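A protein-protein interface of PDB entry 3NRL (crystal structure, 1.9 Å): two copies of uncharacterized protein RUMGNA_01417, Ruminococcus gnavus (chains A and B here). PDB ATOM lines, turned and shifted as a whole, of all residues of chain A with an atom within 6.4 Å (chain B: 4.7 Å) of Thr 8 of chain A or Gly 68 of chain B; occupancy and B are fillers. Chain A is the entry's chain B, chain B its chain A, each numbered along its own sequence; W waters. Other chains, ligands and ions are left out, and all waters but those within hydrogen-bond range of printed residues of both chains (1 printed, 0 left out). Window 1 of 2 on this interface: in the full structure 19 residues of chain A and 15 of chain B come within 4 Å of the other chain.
Printed residues of chain A that touch a printed residue of chain B: Glu 6, Gly 7, Thr 8, Phe 10, Arg 21, Gly 68 and Arg 70. Among the printed residues, 12 pairs touch across the chains. Among the printed residues, no Asp or Glu carboxylate lies within 4 Å of a Lys or Arg side-chain nitrogen of the other chain.
The backbone carbonyl oxygen of Leu 9 of chain B lies within hydrogen-bond range of the backbone NH of Gly 68 of chain B (2.9 Å). The backbone carbonyl oxygen (O) of Leu 69 of chain B lies within hydrogen-bond range of the backbone NH (N) of Leu 9 of chain B, at 2.9 Å. The side-chain carboxylate of Glu 6 of chain A lies within salt-bridge range of the guanidinium group of Arg 70 of chain A (2.8 Å). The backbone NH (N) of Gly 7 of chain A sits at hydrogen-bond distance from the backbone carbonyl oxygen (O) of Val 71 of chain A (2.9 Å). The backbone NH (N) of Arg 21 of chain A sits at hydrogen-bond distance from the backbone carbonyl oxygen (O) of Thr 8 of chain A. The backbone carbonyl oxygen of Phe 10 of chain A sits at hydrogen-bond distance from the backbone NH of Asp 19 of chain A (2.8 Å).
The side-chain hydroxyl (OG1) of Thr 8 of chain B lies within hydrogen-bond range of the backbone carbonyl oxygen (O) of Gly 68 of chain A (2.5 Å). NH2 of Arg 21 of chain A sits at hydrogen-bond distance from O of Asp 67 of chain B, 2.8 Å away. OG1 of Thr 8 of chain A sits at hydrogen-bond distance from O of Gly 68 of chain B (2.4 Å). The backbone carbonyl oxygen (O) of Gly 68 of chain B sits close to the guanidinium group (NE) of Arg 21 of chain A, at 3.5 Å. The guanidinium group (NE) of Arg 21 of chain A lies close to the backbone NH (N) of Leu 69 of chain B, 3.3 Å away.
Water W1 lies within hydrogen-bond range of the guanidinium group of Arg 70 of chain B (3.0 Å) and the backbone carbonyl oxygen of Arg 21 of chain A (3.2 Å).
Printed residues of chain B within 4 Å of Phe 10 of chain A: Asp 67 (3.4 Å). Printed residues of chain B within 4 Å of Arg 21 of chain A: Leu 66 (3.9 Å), Asp 67 (2.8 Å), Gly 68 (3.2 Å) and Leu 69 (3.3 Å). Of the printed residues of chain B, Gly 68 of chain A touches Thr 8. Of the printed residues of chain A, Thr 8 of chain B touches Thr 8 and Gly 68. Printed residues of chain A within 4 Å of Gly 68 of chain B: Thr 8 (2.4 Å) and Arg 21 (3.2 Å). Printed residues of chain A within 4 Å of Arg 70 of chain B: Glu 6 (3.99 Å), Gly 7 (3.5 Å), Thr 8 (3.8 Å) and Arg 70 (3.6 Å). The nearest printed residue of chain B that does not touch Arg 70 of chain A is Thr 8 of chain B (4.2 Å).
Thr 8 of chain A touches its own counterpart, Thr 8 of chain B. Thr 8 of chain A touches Gly 68 of chain B, and with the chains exchanged Gly 68 of chain A touches Thr 8 of chain B. Thr 8 of chain A touches Arg 70 of chain B, but with the chains exchanged Arg 70 of chain A does not touch Thr 8 of chain B (4.2 Å). Arg 70 of chain B touches its own counterpart, Arg 70 of chain A. 5 positions are printed for both chains. Of the 12 pairs that touch across the chains among the printed residues, 4 have their exchanged pair printed and touching as well.
CB of Glu 6 of chain A touches NH2 of Arg 70 of chain B, at 3.99 Å. O of Gly 7 of chain A touches NH2 of Arg 70 of chain B, 3.5 Å away. Thr 8 of chain A touches Thr 8 of chain B (CG2 to CG2, 3.6 Å). Thr 8 of chain A touches Arg 70 of chain B (CG2 to NE, 3.8 Å). CD1 of Phe 10 of chain A touches CB of Asp 67 of chain B (3.4 Å). Arg 21 of chain A touches Leu 66 of chain B (NH2 to C, 3.9 Å). Arg 70 of chain A touches Arg 70 of chain B.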
ATOM      1  N   GLU A   6      -9.422  -5.428   6.808  1.00  0.00           N
ATOM      2  CA  GLU A   6      -8.820  -5.333   8.130  1.00  0.00           C
ATOM      3  C   GLU A   6      -8.042  -6.613   8.400  1.00  0.00           C
ATOM      4  O   GLU A   6      -8.387  -7.683   7.893  1.00  0.00           O
ATOM      5  CB  GLU A   6      -9.897  -5.127   9.197  1.00  0.00           C
ATOM      6  CG  GLU A   6     -10.572  -3.766   9.107  1.00  0.00           C
ATOM      7  CD  GLU A   6     -11.627  -3.552  10.172  1.00  0.00           C
ATOM      8  OE1 GLU A   6     -11.350  -3.844  11.356  1.00  0.00           O
ATOM      9  OE2 GLU A   6     -12.729  -3.076   9.824  1.00  0.00           O
ATOM     10  N   GLY A   7      -6.975  -6.497   9.177  1.00  0.00           N
ATOM     11  CA  GLY A   7      -6.180  -7.672   9.475  1.00  0.00           C
ATOM     12  C   GLY A   7      -5.265  -7.439  10.649  1.00  0.00           C
ATOM     13  O   GLY A   7      -5.398  -6.449  11.367  1.00  0.00           O
ATOM     14  N   THR A   8      -4.323  -8.354  10.839  1.00  0.00           N
ATOM     15  CA  THR A   8      -3.388  -8.234  11.941  1.00  0.00           C
ATOM     16  C   THR A   8      -1.959  -8.223  11.418  1.00  0.00           C
ATOM     17  O   THR A   8      -1.616  -8.966  10.500  1.00  0.00           O
ATOM     18  CB  THR A   8      -3.554  -9.396  12.921  1.00  0.00           C
ATOM     19  OG1 THR A   8      -3.321 -10.627  12.231  1.00  0.00           O
ATOM     20  CG2 THR A   8      -4.961  -9.404  13.489  1.00  0.00           C
ATOM     21  N   LEU A   9      -1.143  -7.360  12.012  1.00  0.00           N
ATOM     22  CA  LEU A   9       0.260  -7.207  11.643  1.00  0.00           C
ATOM     23  C   LEU A   9       1.092  -8.207  12.446  1.00  0.00           C
ATOM     24  O   LEU A   9       0.919  -8.325  13.658  1.00  0.00           O
ATOM     25  CB  LEU A   9       0.720  -5.784  11.964  1.00  0.00           C
ATOM     26  CG  LEU A   9       2.109  -5.369  11.481  1.00  0.00           C
ATOM     27  CD1 LEU A   9       2.123  -5.329   9.951  1.00  0.00           C
ATOM     28  CD2 LEU A   9       2.455  -3.998  12.055  1.00  0.00           C
ATOM     29  N   PHE A  10       1.984  -8.927  11.771  1.00  0.00           N
ATOM     30  CA  PHE A  10       2.824  -9.911  12.451  1.00  0.00           C
ATOM     31  C   PHE A  10       4.173 -10.063  11.750  1.00  0.00           C
ATOM     32  O   PHE A  10       4.302  -9.762  10.565  1.00  0.00           O
ATOM     33  CB  PHE A  10       2.103 -11.261  12.520  1.00  0.00           C
ATOM     34  CG  PHE A  10       2.000 -11.967  11.199  1.00  0.00           C
ATOM     35  CD1 PHE A  10       2.967 -12.898  10.819  1.00  0.00           C
ATOM     36  CD2 PHE A  10       0.957 -11.685  10.322  1.00  0.00           C
ATOM     37  CE1 PHE A  10       2.897 -13.538   9.586  1.00  0.00           C
ATOM     38  CE2 PHE A  10       0.874 -12.320   9.076  1.00  0.00           C
ATOM     39  CZ  PHE A  10       1.851 -13.251   8.707  1.00  0.00           C
ATOM     40  N   ASP A  19       4.102  -8.743   7.981  1.00  0.00           N
ATOM     41  CA  ASP A  19       3.072  -9.065   7.012  1.00  0.00           C
ATOM     42  C   ASP A  19       1.722  -8.856   7.684  1.00  0.00           C
ATOM     43  O   ASP A  19       1.652  -8.618   8.889  1.00  0.00           O
ATOM     44  CB  ASP A  19       3.228 -10.518   6.544  1.00  0.00           C
ATOM     45  CG  ASP A  19       2.426 -10.819   5.281  1.00  0.00           C
ATOM     46  OD1 ASP A  19       1.921  -9.870   4.648  1.00  0.00           O
ATOM     47  OD2 ASP A  19       2.308 -12.008   4.915  1.00  0.00           O
ATOM     48  N   ILE A  20       0.659  -8.936   6.900  1.00  0.00           N
ATOM     49  CA  ILE A  20      -0.675  -8.752   7.432  1.00  0.00           C
ATOM     50  C   ILE A  20      -1.514  -9.987   7.148  1.00  0.00           C
ATOM     51  O   ILE A  20      -1.526 -10.493   6.024  1.00  0.00           O
ATOM     52  CB  ILE A  20      -1.368  -7.539   6.789  1.00  0.00           C
ATOM     53  CG1 ILE A  20      -0.547  -6.271   7.049  1.00  0.00           C
ATOM     54  CG2 ILE A  20      -2.782  -7.392   7.351  1.00  0.00           C
ATOM     55  CD1 ILE A  20      -1.011  -5.077   6.230  1.00  0.00           C
ATOM     56  N   ARG A  21      -2.193 -10.478   8.177  1.00  0.00           N
ATOM     57  CA  ARG A  21      -3.070 -11.628   8.027  1.00  0.00           C
ATOM     58  C   ARG A  21      -4.488 -11.065   7.970  1.00  0.00           C
ATOM     59  O   ARG A  21      -4.977 -10.516   8.953  1.00  0.00           O
ATOM     60  CB  ARG A  21      -2.938 -12.563   9.222  1.00  0.00           C
ATOM     61  CG  ARG A  21      -3.857 -13.764   9.139  1.00  0.00           C
ATOM     62  CD  ARG A  21      -4.184 -14.256  10.537  1.00  0.00           C
ATOM     63  NE  ARG A  21      -3.193 -15.194  11.050  1.00  0.00           N
ATOM     64  CZ  ARG A  21      -3.010 -16.411  10.551  1.00  0.00           C
ATOM     65  NH1 ARG A  21      -3.754 -16.798   9.532  1.00  0.00           N
ATOM     66  NH2 ARG A  21      -2.114 -17.241  11.083  1.00  0.00           N
ATOM     67  N   PHE A  22      -5.137 -11.200   6.819  1.00  0.00           N
ATOM     68  CA  PHE A  22      -6.492 -10.692   6.634  1.00  0.00           C
ATOM     69  C   PHE A  22      -7.554 -11.690   7.085  1.00  0.00           C
ATOM     70  O   PHE A  22      -8.533 -11.319   7.723  1.00  0.00           O
ATOM     71  CB  PHE A  22      -6.711 -10.324   5.161  1.00  0.00           C
ATOM     72  CG  PHE A  22      -5.901  -9.135   4.705  1.00  0.00           C
ATOM     73  CD1 PHE A  22      -6.114  -7.879   5.265  1.00  0.00           C
ATOM     74  CD2 PHE A  22      -4.918  -9.273   3.730  1.00  0.00           C
ATOM     75  CE1 PHE A  22      -5.356  -6.780   4.864  1.00  0.00           C
ATOM     76  CE2 PHE A  22      -4.153  -8.176   3.320  1.00  0.00           C
ATOM     77  CZ  PHE A  22      -4.374  -6.930   3.889  1.00  0.00           C
ATOM     78  N   GLY A  68       1.265  -7.870  16.437  1.00  0.00           N
ATOM     79  CA  GLY A  68      -0.103  -7.947  16.922  1.00  0.00           C
ATOM     80  C   GLY A  68      -1.006  -6.744  16.735  1.00  0.00           C
ATOM     81  O   GLY A  68      -2.172  -6.778  17.135  1.00  0.00           O
ATOM     82  N   LEU A  69      -0.488  -5.680  16.138  1.00  0.00           N
ATOM     83  CA  LEU A  69      -1.315  -4.499  15.923  1.00  0.00           C
ATOM     84  C   LEU A  69      -2.445  -4.825  14.955  1.00  0.00           C
ATOM     85  O   LEU A  69      -2.273  -5.638  14.041  1.00  0.00           O
ATOM     86  CB  LEU A  69      -0.478  -3.360  15.342  1.00  0.00           C
ATOM     87  CG  LEU A  69       0.576  -2.720  16.253  1.00  0.00           C
ATOM     88  CD1 LEU A  69       1.348  -1.666  15.456  1.00  0.00           C
ATOM     89  CD2 LEU A  69      -0.095  -2.086  17.468  1.00  0.00           C
ATOM     90  N   ARG A  70      -3.605  -4.211  15.172  1.00  0.00           N
ATOM     91  CA  ARG A  70      -4.733  -4.386  14.265  1.00  0.00           C
ATOM     92  C   ARG A  70      -4.546  -3.304  13.207  1.00  0.00           C
ATOM     93  O   ARG A  70      -4.262  -2.148  13.527  1.00  0.00           O
ATOM     94  CB  ARG A  70      -6.064  -4.183  14.988  1.00  0.00           C
ATOM     95  CG  ARG A  70      -6.490  -5.354  15.857  1.00  0.00           C
ATOM     96  CD  ARG A  70      -7.944  -5.189  16.267  1.00  0.00           C
ATOM     97  NE  ARG A  70      -8.796  -4.974  15.098  1.00  0.00           N
ATOM     98  CZ  ARG A  70     -10.100  -4.729  15.150  1.00  0.00           C
ATOM     99  NH1 ARG A  70     -10.720  -4.665  16.320  1.00  0.00           N
ATOM    100  NH2 ARG A  70     -10.785  -4.544  14.028  1.00  0.00           N
ATOM    101  N   VAL A  71      -4.691  -3.680  11.946  1.00  0.00           N
ATOM    102  CA  VAL A  71      -4.490  -2.733  10.864  1.00  0.00           C
ATOM    103  C   VAL A  71      -5.546  -2.863   9.782  1.00  0.00           C
ATOM    104  O   VAL A  71      -6.364  -3.783   9.803  1.00  0.00           O
ATOM    105  CB  VAL A  71      -3.109  -2.944  10.218  1.00  0.00           C
ATOM    106  CG1 VAL A  71      -2.011  -2.780  11.278  1.00  0.00           C
ATOM    107  CG2 VAL A  71      -3.047  -4.335   9.579  1.00  0.00           C
ATOM    108  N   THR B   8      -4.712 -10.288  19.684  1.00  0.00           N
ATOM    109  CA  THR B   8      -4.052 -10.876  18.530  1.00  0.00           C
ATOM    110  C   THR B   8      -2.884 -11.722  19.000  1.00  0.00           C
ATOM    111  O   THR B   8      -2.115 -11.309  19.870  1.00  0.00           O
ATOM    112  CB  THR B   8      -3.530  -9.791  17.586  1.00  0.00           C
ATOM    113  OG1 THR B   8      -2.668  -8.910  18.312  1.00  0.00           O
ATOM    114  CG2 THR B   8      -4.678  -8.997  17.015  1.00  0.00           C
ATOM    115  N   LEU B   9      -2.766 -12.907  18.416  1.00  0.00           N
ATOM    116  CA  LEU B   9      -1.716 -13.862  18.756  1.00  0.00           C
ATOM    117  C   LEU B   9      -0.444 -13.584  17.958  1.00  0.00           C
ATOM    118  O   LEU B   9      -0.497 -13.335  16.748  1.00  0.00           O
ATOM    119  CB  LEU B   9      -2.226 -15.282  18.471  1.00  0.00           C
ATOM    120  CG  LEU B   9      -1.410 -16.491  18.925  1.00  0.00           C
ATOM    121  CD1 LEU B   9      -1.349 -16.552  20.454  1.00  0.00           C
ATOM    122  CD2 LEU B   9      -2.046 -17.754  18.370  1.00  0.00           C
ATOM    123  N   LEU B  66       0.462 -19.915  13.461  1.00  0.00           N
ATOM    124  CA  LEU B  66      -0.254 -19.240  14.543  1.00  0.00           C
ATOM    125  C   LEU B  66      -0.180 -17.712  14.491  1.00  0.00           C
ATOM    126  O   LEU B  66      -1.010 -17.018  15.074  1.00  0.00           O
ATOM    127  CB  LEU B  66       0.292 -19.710  15.901  1.00  0.00           C
ATOM    128  CG  LEU B  66      -0.166 -21.060  16.460  1.00  0.00           C
ATOM    129  CD1 LEU B  66       0.144 -22.166  15.465  1.00  0.00           C
ATOM    130  CD2 LEU B  66       0.527 -21.328  17.794  1.00  0.00           C
ATOM    131  N   ASP B  67       0.814 -17.194  13.786  1.00  0.00           N
ATOM    132  CA  ASP B  67       1.032 -15.754  13.707  1.00  0.00           C
ATOM    133  C   ASP B  67      -0.110 -14.910  13.162  1.00  0.00           C
ATOM    134  O   ASP B  67      -0.591 -15.134  12.055  1.00  0.00           O
ATOM    135  CB  ASP B  67       2.285 -15.492  12.879  1.00  0.00           C
ATOM    136  CG  ASP B  67       3.380 -16.492  13.174  1.00  0.00           C
ATOM    137  OD1 ASP B  67       4.051 -16.356  14.220  1.00  0.00           O
ATOM    138  OD2 ASP B  67       3.551 -17.427  12.362  1.00  0.00           O
ATOM    139  N   GLY B  68      -0.526 -13.924  13.951  1.00  0.00           N
ATOM    140  CA  GLY B  68      -1.571 -13.017  13.521  1.00  0.00           C
ATOM    141  C   GLY B  68      -3.012 -13.432  13.719  1.00  0.00           C
ATOM    142  O   GLY B  68      -3.914 -12.696  13.339  1.00  0.00           O
ATOM    143  N   LEU B  69      -3.249 -14.601  14.301  1.00  0.00           N
ATOM    144  CA  LEU B  69      -4.622 -15.044  14.514  1.00  0.00           C
ATOM    145  C   LEU B  69      -5.323 -14.131  15.515  1.00  0.00           C
ATOM    146  O   LEU B  69      -4.689 -13.592  16.423  1.00  0.00           O
ATOM    147  CB  LEU B  69      -4.640 -16.471  15.060  1.00  0.00           C
ATOM    148  CG  LEU B  69      -4.197 -17.611  14.144  1.00  0.00           C
ATOM    149  CD1 LEU B  69      -4.120 -18.906  14.943  1.00  0.00           C
ATOM    150  CD2 LEU B  69      -5.190 -17.761  12.989  1.00  0.00           C
ATOM    151  N   ARG B  70      -6.628 -13.942  15.343  1.00  0.00           N
ATOM    152  CA  ARG B  70      -7.386 -13.135  16.291  1.00  0.00           C
ATOM    153  C   ARG B  70      -7.884 -14.121  17.325  1.00  0.00           C
ATOM    154  O   ARG B  70      -8.448 -15.160  16.977  1.00  0.00           O
ATOM    155  CB  ARG B  70      -8.556 -12.422  15.603  1.00  0.00           C
ATOM    156  CG  ARG B  70      -8.198 -11.006  15.177  1.00  0.00           C
ATOM    157  CD  ARG B  70      -9.057 -10.500  14.033  1.00  0.00           C
ATOM    158  NE  ARG B  70      -8.743  -9.110  13.708  1.00  0.00           N
ATOM    159  CZ  ARG B  70      -9.024  -8.525  12.547  1.00  0.00           C
ATOM    160  NH1 ARG B  70      -9.626  -9.208  11.580  1.00  0.00           N
ATOM    161  NH2 ARG B  70      -8.703  -7.254  12.355  1.00  0.00           N
HETATM  162  O   HOH W   1      -7.235 -11.003  11.157  1.00  0.00           O
